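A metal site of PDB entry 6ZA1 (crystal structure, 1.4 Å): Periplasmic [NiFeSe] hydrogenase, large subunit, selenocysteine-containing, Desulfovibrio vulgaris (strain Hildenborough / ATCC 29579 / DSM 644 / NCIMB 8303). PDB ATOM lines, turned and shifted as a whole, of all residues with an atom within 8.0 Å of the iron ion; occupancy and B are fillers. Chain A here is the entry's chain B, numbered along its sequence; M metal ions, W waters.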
ATOM      1  N   TYR A  41      27.809  19.134   8.023  1.00  0.00           N
ATOM      2  CA  TYR A  41      26.490  18.534   7.934  1.00  0.00           C
ATOM      3  C   TYR A  41      25.996  18.134   9.320  1.00  0.00           C
ATOM      4  O   TYR A  41      26.762  17.623  10.143  1.00  0.00           O
ATOM      5  CB  TYR A  41      26.559  17.276   7.048  1.00  0.00           C
ATOM      6  CG  TYR A  41      25.285  16.452   6.976  1.00  0.00           C
ATOM      7  CD1 TYR A  41      24.264  16.794   6.117  1.00  0.00           C
ATOM      8  CD2 TYR A  41      25.124  15.319   7.771  1.00  0.00           C
ATOM      9  CE1 TYR A  41      23.103  16.051   6.036  1.00  0.00           C
ATOM     10  CE2 TYR A  41      23.962  14.555   7.702  1.00  0.00           C
ATOM     11  CZ  TYR A  41      22.960  14.931   6.827  1.00  0.00           C
ATOM     12  OH  TYR A  41      21.791  14.202   6.729  1.00  0.00           O
ATOM     13  N   GLU A  45      16.870  16.953   8.713  1.00  0.00           N
ATOM     14  CA  GLU A  45      15.758  16.261   8.077  1.00  0.00           C
ATOM     15  C   GLU A  45      15.567  14.859   8.638  1.00  0.00           C
ATOM     16  O   GLU A  45      14.434  14.358   8.637  1.00  0.00           O
ATOM     17  CB  GLU A  45      15.947  16.295   6.562  1.00  0.00           C
ATOM     18  CG  GLU A  45      15.767  17.727   6.016  1.00  0.00           C
ATOM     19  CD  GLU A  45      16.498  18.008   4.705  1.00  0.00           C
ATOM     20  OE1 GLU A  45      17.499  17.316   4.416  1.00  0.00           O
ATOM     21  OE2 GLU A  45      16.072  18.938   3.979  1.00  0.00           O
ATOM     22  N   ILE A  63      18.814  25.292  12.852  1.00  0.00           N
ATOM     23  CA  ILE A  63      19.558  25.261  11.596  1.00  0.00           C
ATOM     24  C   ILE A  63      20.525  26.429  11.530  1.00  0.00           C
ATOM     25  O   ILE A  63      21.652  26.299  11.031  1.00  0.00           O
ATOM     26  CB  ILE A  63      18.600  25.235  10.388  1.00  0.00           C
ATOM     27  CG1 ILE A  63      17.875  23.881  10.338  1.00  0.00           C
ATOM     28  CG2 ILE A  63      19.354  25.528   9.098  1.00  0.00           C
ATOM     29  CD1 ILE A  63      16.709  23.836   9.390  1.00  0.00           C
ATOM     30  N   GLU A 271      15.714  18.470  -6.388  1.00  0.00           N
ATOM     31  CA  GLU A 271      17.038  18.529  -5.777  1.00  0.00           C
ATOM     32  C   GLU A 271      17.906  17.391  -6.310  1.00  0.00           C
ATOM     33  O   GLU A 271      17.558  16.216  -6.148  1.00  0.00           O
ATOM     34  CB  GLU A 271      16.950  18.485  -4.248  1.00  0.00           C
ATOM     35  CG  GLU A 271      16.319  19.737  -3.650  1.00  0.00           C
ATOM     36  CD  GLU A 271      16.486  19.795  -2.145  1.00  0.00           C
ATOM     37  OE1 GLU A 271      15.704  19.126  -1.431  1.00  0.00           O
ATOM     38  OE2 GLU A 271      17.390  20.508  -1.683  1.00  0.00           O
ATOM     39  N   PHE A 278      25.476  12.701  -0.954  1.00  0.00           N
ATOM     40  CA  PHE A 278      24.247  11.980  -0.649  1.00  0.00           C
ATOM     41  C   PHE A 278      24.124  10.802  -1.598  1.00  0.00           C
ATOM     42  O   PHE A 278      24.706  10.786  -2.687  1.00  0.00           O
ATOM     43  CB  PHE A 278      23.017  12.907  -0.738  1.00  0.00           C
ATOM     44  CG  PHE A 278      23.092  14.034   0.237  1.00  0.00           C
ATOM     45  CD1 PHE A 278      22.759  13.821   1.558  1.00  0.00           C
ATOM     46  CD2 PHE A 278      23.577  15.273  -0.143  1.00  0.00           C
ATOM     47  CE1 PHE A 278      22.872  14.836   2.483  1.00  0.00           C
ATOM     48  CE2 PHE A 278      23.691  16.301   0.781  1.00  0.00           C
ATOM     49  CZ  PHE A 278      23.337  16.069   2.094  1.00  0.00           C
ATOM     50  N   TYR A 287      10.721  18.175  -3.219  1.00  0.00           N
ATOM     51  CA  TYR A 287      10.792  18.170  -1.753  1.00  0.00           C
ATOM     52  C   TYR A 287       9.682  17.337  -1.119  1.00  0.00           C
ATOM     53  O   TYR A 287       9.881  16.793  -0.023  1.00  0.00           O
ATOM     54  CB  TYR A 287      10.800  19.613  -1.221  1.00  0.00           C
ATOM     55  CG  TYR A 287       9.596  20.394  -1.694  1.00  0.00           C
ATOM     56  CD1 TYR A 287       8.395  20.304  -1.022  1.00  0.00           C
ATOM     57  CD2 TYR A 287       9.666  21.195  -2.821  1.00  0.00           C
ATOM     58  CE1 TYR A 287       7.295  20.984  -1.450  1.00  0.00           C
ATOM     59  CE2 TYR A 287       8.558  21.876  -3.264  1.00  0.00           C
ATOM     60  CZ  TYR A 287       7.377  21.770  -2.571  1.00  0.00           C
ATOM     61  OH  TYR A 287       6.275  22.457  -3.011  1.00  0.00           O
ATOM     62  N   GLY A 290      11.250  14.189  -0.808  1.00  0.00           N
ATOM     63  CA  GLY A 290      12.664  14.345  -0.561  1.00  0.00           C
ATOM     64  C   GLY A 290      13.198  13.294   0.400  1.00  0.00           C
ATOM     65  O   GLY A 290      12.476  12.751   1.241  1.00  0.00           O
ATOM     66  N   LYS A 291      14.477  12.999   0.238  1.00  0.00           N
ATOM     67  CA  LYS A 291      15.165  12.041   1.085  1.00  0.00           C
ATOM     68  C   LYS A 291      16.568  12.569   1.351  1.00  0.00           C
ATOM     69  O   LYS A 291      17.179  13.207   0.495  1.00  0.00           O
ATOM     70  CB  LYS A 291      15.351  10.694   0.403  1.00  0.00           C
ATOM     71  CG  LYS A 291      14.104   9.975   0.004  1.00  0.00           C
ATOM     72  CD  LYS A 291      14.505   8.594  -0.489  1.00  0.00           C
ATOM     73  CE  LYS A 291      13.311   7.738  -0.808  1.00  0.00           C
ATOM     74  NZ  LYS A 291      12.480   7.555   0.416  1.00  0.00           N
ATOM     75  N   THR A 292      17.081  12.275   2.536  1.00  0.00           N
ATOM     76  CA  THR A 292      18.395  12.769   2.973  1.00  0.00           C
ATOM     77  C   THR A 292      19.180  11.583   3.521  1.00  0.00           C
ATOM     78  O   THR A 292      18.976  11.166   4.665  1.00  0.00           O
ATOM     79  CB  THR A 292      18.215  13.900   3.975  1.00  0.00           C
ATOM     80  OG1 THR A 292      17.367  14.890   3.360  1.00  0.00           O
ATOM     81  CG2 THR A 292      19.550  14.510   4.334  1.00  0.00           C
ATOM     82  N   PHE A 304      28.151  19.161   0.866  1.00  0.00           N
ATOM     83  CA  PHE A 304      26.965  18.701   1.577  1.00  0.00           C
ATOM     84  C   PHE A 304      25.709  19.484   1.201  1.00  0.00           C
ATOM     85  O   PHE A 304      24.624  19.192   1.722  1.00  0.00           O
ATOM     86  CB  PHE A 304      27.189  18.769   3.095  1.00  0.00           C
ATOM     87  CG  PHE A 304      28.095  17.685   3.635  1.00  0.00           C
ATOM     88  CD1 PHE A 304      27.722  16.346   3.556  1.00  0.00           C
ATOM     89  CD2 PHE A 304      29.294  17.998   4.255  1.00  0.00           C
ATOM     90  CE1 PHE A 304      28.549  15.347   4.062  1.00  0.00           C
ATOM     91  CE2 PHE A 304      30.121  16.999   4.761  1.00  0.00           C
ATOM     92  CZ  PHE A 304      29.740  15.675   4.667  1.00  0.00           C
ATOM     93  N   VAL A 305      25.815  20.461   0.295  1.00  0.00           N
ATOM     94  CA  VAL A 305      24.663  21.186  -0.215  1.00  0.00           C
ATOM     95  C   VAL A 305      24.102  20.397  -1.397  1.00  0.00           C
ATOM     96  O   VAL A 305      24.856  20.030  -2.311  1.00  0.00           O
ATOM     97  CB  VAL A 305      25.074  22.607  -0.656  1.00  0.00           C
ATOM     98  CG1 VAL A 305      23.865  23.443  -1.025  1.00  0.00           C
ATOM     99  CG2 VAL A 305      25.865  23.300   0.452  1.00  0.00           C
ATOM    100  N   LYS A 306      22.809  20.098  -1.356  1.00  0.00           N
ATOM    101  CA  LYS A 306      22.154  19.532  -2.533  1.00  0.00           C
ATOM    102  C   LYS A 306      22.054  20.607  -3.618  1.00  0.00           C
ATOM    103  O   LYS A 306      22.283  21.789  -3.372  1.00  0.00           O
ATOM    104  CB  LYS A 306      20.749  19.029  -2.184  1.00  0.00           C
ATOM    105  CG  LYS A 306      20.687  17.851  -1.208  1.00  0.00           C
ATOM    106  CD  LYS A 306      19.228  17.473  -0.905  1.00  0.00           C
ATOM    107  CE  LYS A 306      19.113  16.315   0.089  1.00  0.00           C
ATOM    108  NZ  LYS A 306      17.715  16.086   0.539  1.00  0.00           N
ATOM    109  N   LEU A 415      11.539  27.094   1.999  1.00  0.00           N
ATOM    110  CA  LEU A 415      10.338  26.301   2.180  1.00  0.00           C
ATOM    111  C   LEU A 415      10.647  25.142   3.103  1.00  0.00           C
ATOM    112  O   LEU A 415      11.762  24.600   3.118  1.00  0.00           O
ATOM    113  CB  LEU A 415       9.763  25.799   0.857  1.00  0.00           C
ATOM    114  CG  LEU A 415      10.544  24.705   0.115  1.00  0.00           C
ATOM    115  CD1 LEU A 415      10.090  23.339   0.575  1.00  0.00           C
ATOM    116  CD2 LEU A 415      10.368  24.882  -1.380  1.00  0.00           C
ATOM    117  N   TYR A 428      10.397  15.470   6.864  1.00  0.00           N
ATOM    118  CA  TYR A 428      10.525  16.919   6.954  1.00  0.00           C
ATOM    119  C   TYR A 428      11.641  17.312   5.997  1.00  0.00           C
ATOM    120  O   TYR A 428      12.761  16.795   6.122  1.00  0.00           O
ATOM    121  CB  TYR A 428      10.875  17.347   8.379  1.00  0.00           C
ATOM    122  CG  TYR A 428      10.506  18.783   8.695  1.00  0.00           C
ATOM    123  CD1 TYR A 428      11.248  19.849   8.204  1.00  0.00           C
ATOM    124  CD2 TYR A 428       9.403  19.072   9.489  1.00  0.00           C
ATOM    125  CE1 TYR A 428      10.908  21.153   8.501  1.00  0.00           C
ATOM    126  CE2 TYR A 428       9.052  20.370   9.792  1.00  0.00           C
ATOM    127  CZ  TYR A 428       9.806  21.413   9.287  1.00  0.00           C
ATOM    128  OH  TYR A 428       9.445  22.705   9.597  1.00  0.00           O
ATOM    129  N   GLN A 429      11.338  18.163   5.025  1.00  0.00           N
ATOM    130  CA  GLN A 429      12.311  18.532   4.016  1.00  0.00           C
ATOM    131  C   GLN A 429      12.436  20.046   3.955  1.00  0.00           C
ATOM    132  O   GLN A 429      11.424  20.764   3.984  1.00  0.00           O
ATOM    133  CB  GLN A 429      11.944  17.944   2.652  1.00  0.00           C
ATOM    134  CG  GLN A 429      12.194  16.437   2.564  1.00  0.00           C
ATOM    135  CD  GLN A 429      13.665  16.075   2.616  1.00  0.00           C
ATOM    136  OE1 GLN A 429      14.509  16.758   2.039  1.00  0.00           O
ATOM    137  NE2 GLN A 429      13.991  14.998   3.330  1.00  0.00           N
ATOM    138  N   ILE A 430      13.676  20.527   3.908  1.00  0.00           N
ATOM    139  CA  ILE A 430      13.982  21.948   3.927  1.00  0.00           C
ATOM    140  C   ILE A 430      14.719  22.287   2.647  1.00  0.00           C
ATOM    141  O   ILE A 430      15.676  21.603   2.271  1.00  0.00           O
ATOM    142  CB  ILE A 430      14.807  22.316   5.177  1.00  0.00           C
ATOM    143  CG1 ILE A 430      13.956  22.087   6.417  1.00  0.00           C
ATOM    144  CG2 ILE A 430      15.275  23.752   5.070  1.00  0.00           C
ATOM    145  CD1 ILE A 430      14.704  21.463   7.562  1.00  0.00           C
ATOM    146  N   VAL A 431      14.257  23.343   1.971  1.00  0.00           N
ATOM    147  CA  VAL A 431      14.897  23.865   0.764  1.00  0.00           C
ATOM    148  C   VAL A 431      15.080  25.345   1.075  1.00  0.00           C
ATOM    149  O   VAL A 431      14.117  26.115   1.076  1.00  0.00           O
ATOM    150  CB  VAL A 431      14.019  23.659  -0.480  1.00  0.00           C
ATOM    151  CG1 VAL A 431      14.695  24.204  -1.728  1.00  0.00           C
ATOM    152  CG2 VAL A 431      13.711  22.167  -0.659  1.00  0.00           C
ATOM    153  N   SER A 432      16.326  25.747   1.356  1.00  0.00           N
ATOM    154  CA  SER A 432      16.617  27.031   1.975  1.00  0.00           C
ATOM    155  C   SER A 432      17.312  27.990   1.010  1.00  0.00           C
ATOM    156  O   SER A 432      17.686  27.631  -0.112  1.00  0.00           O
ATOM    157  CB  SER A 432      17.520  26.806   3.190  1.00  0.00           C
ATOM    158  OG  SER A 432      18.740  26.235   2.737  1.00  0.00           O
ATOM    159  N   LEU A 435      20.984  27.387   0.048  1.00  0.00           N
ATOM    160  CA  LEU A 435      20.955  26.210  -0.814  1.00  0.00           C
ATOM    161  C   LEU A 435      20.831  26.611  -2.283  1.00  0.00           C
ATOM    162  O   LEU A 435      21.550  26.094  -3.146  1.00  0.00           O
ATOM    163  CB  LEU A 435      19.780  25.324  -0.404  1.00  0.00           C
ATOM    164  CG  LEU A 435      19.355  24.225  -1.376  1.00  0.00           C
ATOM    165  CD1 LEU A 435      20.325  23.065  -1.342  1.00  0.00           C
ATOM    166  CD2 LEU A 435      17.938  23.758  -1.047  1.00  0.00           C
ATOM    167  N   CYS A 481      22.404  27.111   6.884  1.00  0.00           N
ATOM    168  CA  CYS A 481      21.115  26.996   6.205  1.00  0.00           C
ATOM    169  C   CYS A 481      21.201  26.106   4.975  1.00  0.00           C
ATOM    170  O   CYS A 481      20.299  25.316   4.696  1.00  0.00           O
ATOM    171  CB  CYS A 481      20.623  28.370   5.765  1.00  0.00           C
ATOM    172  SG  CYS A 481      19.876  29.285   7.077  1.00  0.00           S
ATOM    173  N   ALA A 482      22.277  26.254   4.197  1.00  0.00           N
ATOM    174  CA  ALA A 482      22.362  25.554   2.916  1.00  0.00           C
ATOM    175  C   ALA A 482      22.367  24.047   3.102  1.00  0.00           C
ATOM    176  O   ALA A 482      21.776  23.319   2.299  1.00  0.00           O
ATOM    177  CB  ALA A 482      23.596  26.014   2.151  1.00  0.00           C
ATOM    178  N   VAL A 483      23.013  23.557   4.155  1.00  0.00           N
ATOM    179  CA  VAL A 483      23.197  22.119   4.373  1.00  0.00           C
ATOM    180  C   VAL A 483      22.161  21.555   5.348  1.00  0.00           C
ATOM    181  O   VAL A 483      21.584  20.492   5.097  1.00  0.00           O
ATOM    182  CB  VAL A 483      24.616  21.808   4.882  1.00  0.00           C
ATOM    183  CG1 VAL A 483      24.766  20.298   5.178  1.00  0.00           C
ATOM    184  CG2 VAL A 483      25.693  22.290   3.922  1.00  0.00           C
ATOM    185  N   HIS A 484      21.944  22.233   6.470  1.00  0.00           N
ATOM    186  CA  HIS A 484      21.064  21.757   7.531  1.00  0.00           C
ATOM    187  C   HIS A 484      21.319  20.289   7.893  1.00  0.00           C
ATOM    188  O   HIS A 484      22.490  19.897   8.065  1.00  0.00           O
ATOM    189  CB  HIS A 484      19.567  22.077   7.239  1.00  0.00           C
ATOM    190  CG  HIS A 484      19.111  21.851   5.826  1.00  0.00           C
ATOM    191  ND1 HIS A 484      19.342  22.754   4.807  1.00  0.00           N
ATOM    192  CD2 HIS A 484      18.384  20.841   5.282  1.00  0.00           C
ATOM    193  CE1 HIS A 484      18.808  22.292   3.688  1.00  0.00           C
ATOM    194  NE2 HIS A 484      18.222  21.137   3.948  1.00  0.00           N
ATOM    195  OXT HIS A 484      20.402  19.489   8.050  1.00  0.00           O
HETATM  196 FE    FE M   1      17.185  19.962   2.460  1.00  0.00          FE
HETATM  197  O   HOH W   1      18.827  18.353   2.487  1.00  0.00           O
HETATM  198  O   HOH W   2      18.243  20.872   0.771  1.00  0.00           O
HETATM  199  O   HOH W   3      16.092  18.703   1.031  1.00  0.00           O
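The side-chain amide oxygen (OE1) of Gln 429 sits close to the side-chain carboxylate (OE2) of Glu 45 (3.3 Å).
OE1 of Glu 45 lies within hydrogen-bond range of OG1 of Thr 292 (2.6 Å).
A ring nitrogen (ND1) of His 484 sits at hydrogen-bond distance from the backbone carbonyl oxygen of Cys 481 (2.7 Å).
Within 4 Å of the iron ion: Glu 45, Ile 430 and His 484.
The nearest printed residue that does not touch the iron ion is Glu 271 (4.2 Å).
The side-chain carboxylate (OE2) of Glu 45 is bound to the iron ion, 2.1 Å away.
NE2 of His 484 is bound to the iron ion, at 2.2 Å.
The iron ion is bound by water W2 (2.2 Å).
Water W3 is bound to the iron ion (2.2 Å).
The iron ion is bound by O of Ile 430 (2.2 Å).
Water W1 is bound to the iron ion (2.3 Å).
The iron ion has six donor atoms within binding distance.
Water W3 lies within hydrogen-bond range of OE1 of Glu 271 (2.5 Å), OE1 of Gln 429 (2.7 Å) and NZ of Lys 306 (3.1 Å).
Water W1 bridges OE1 of Glu 45 (2.6 Å) and NZ of Lys 306 (3.2 Å).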
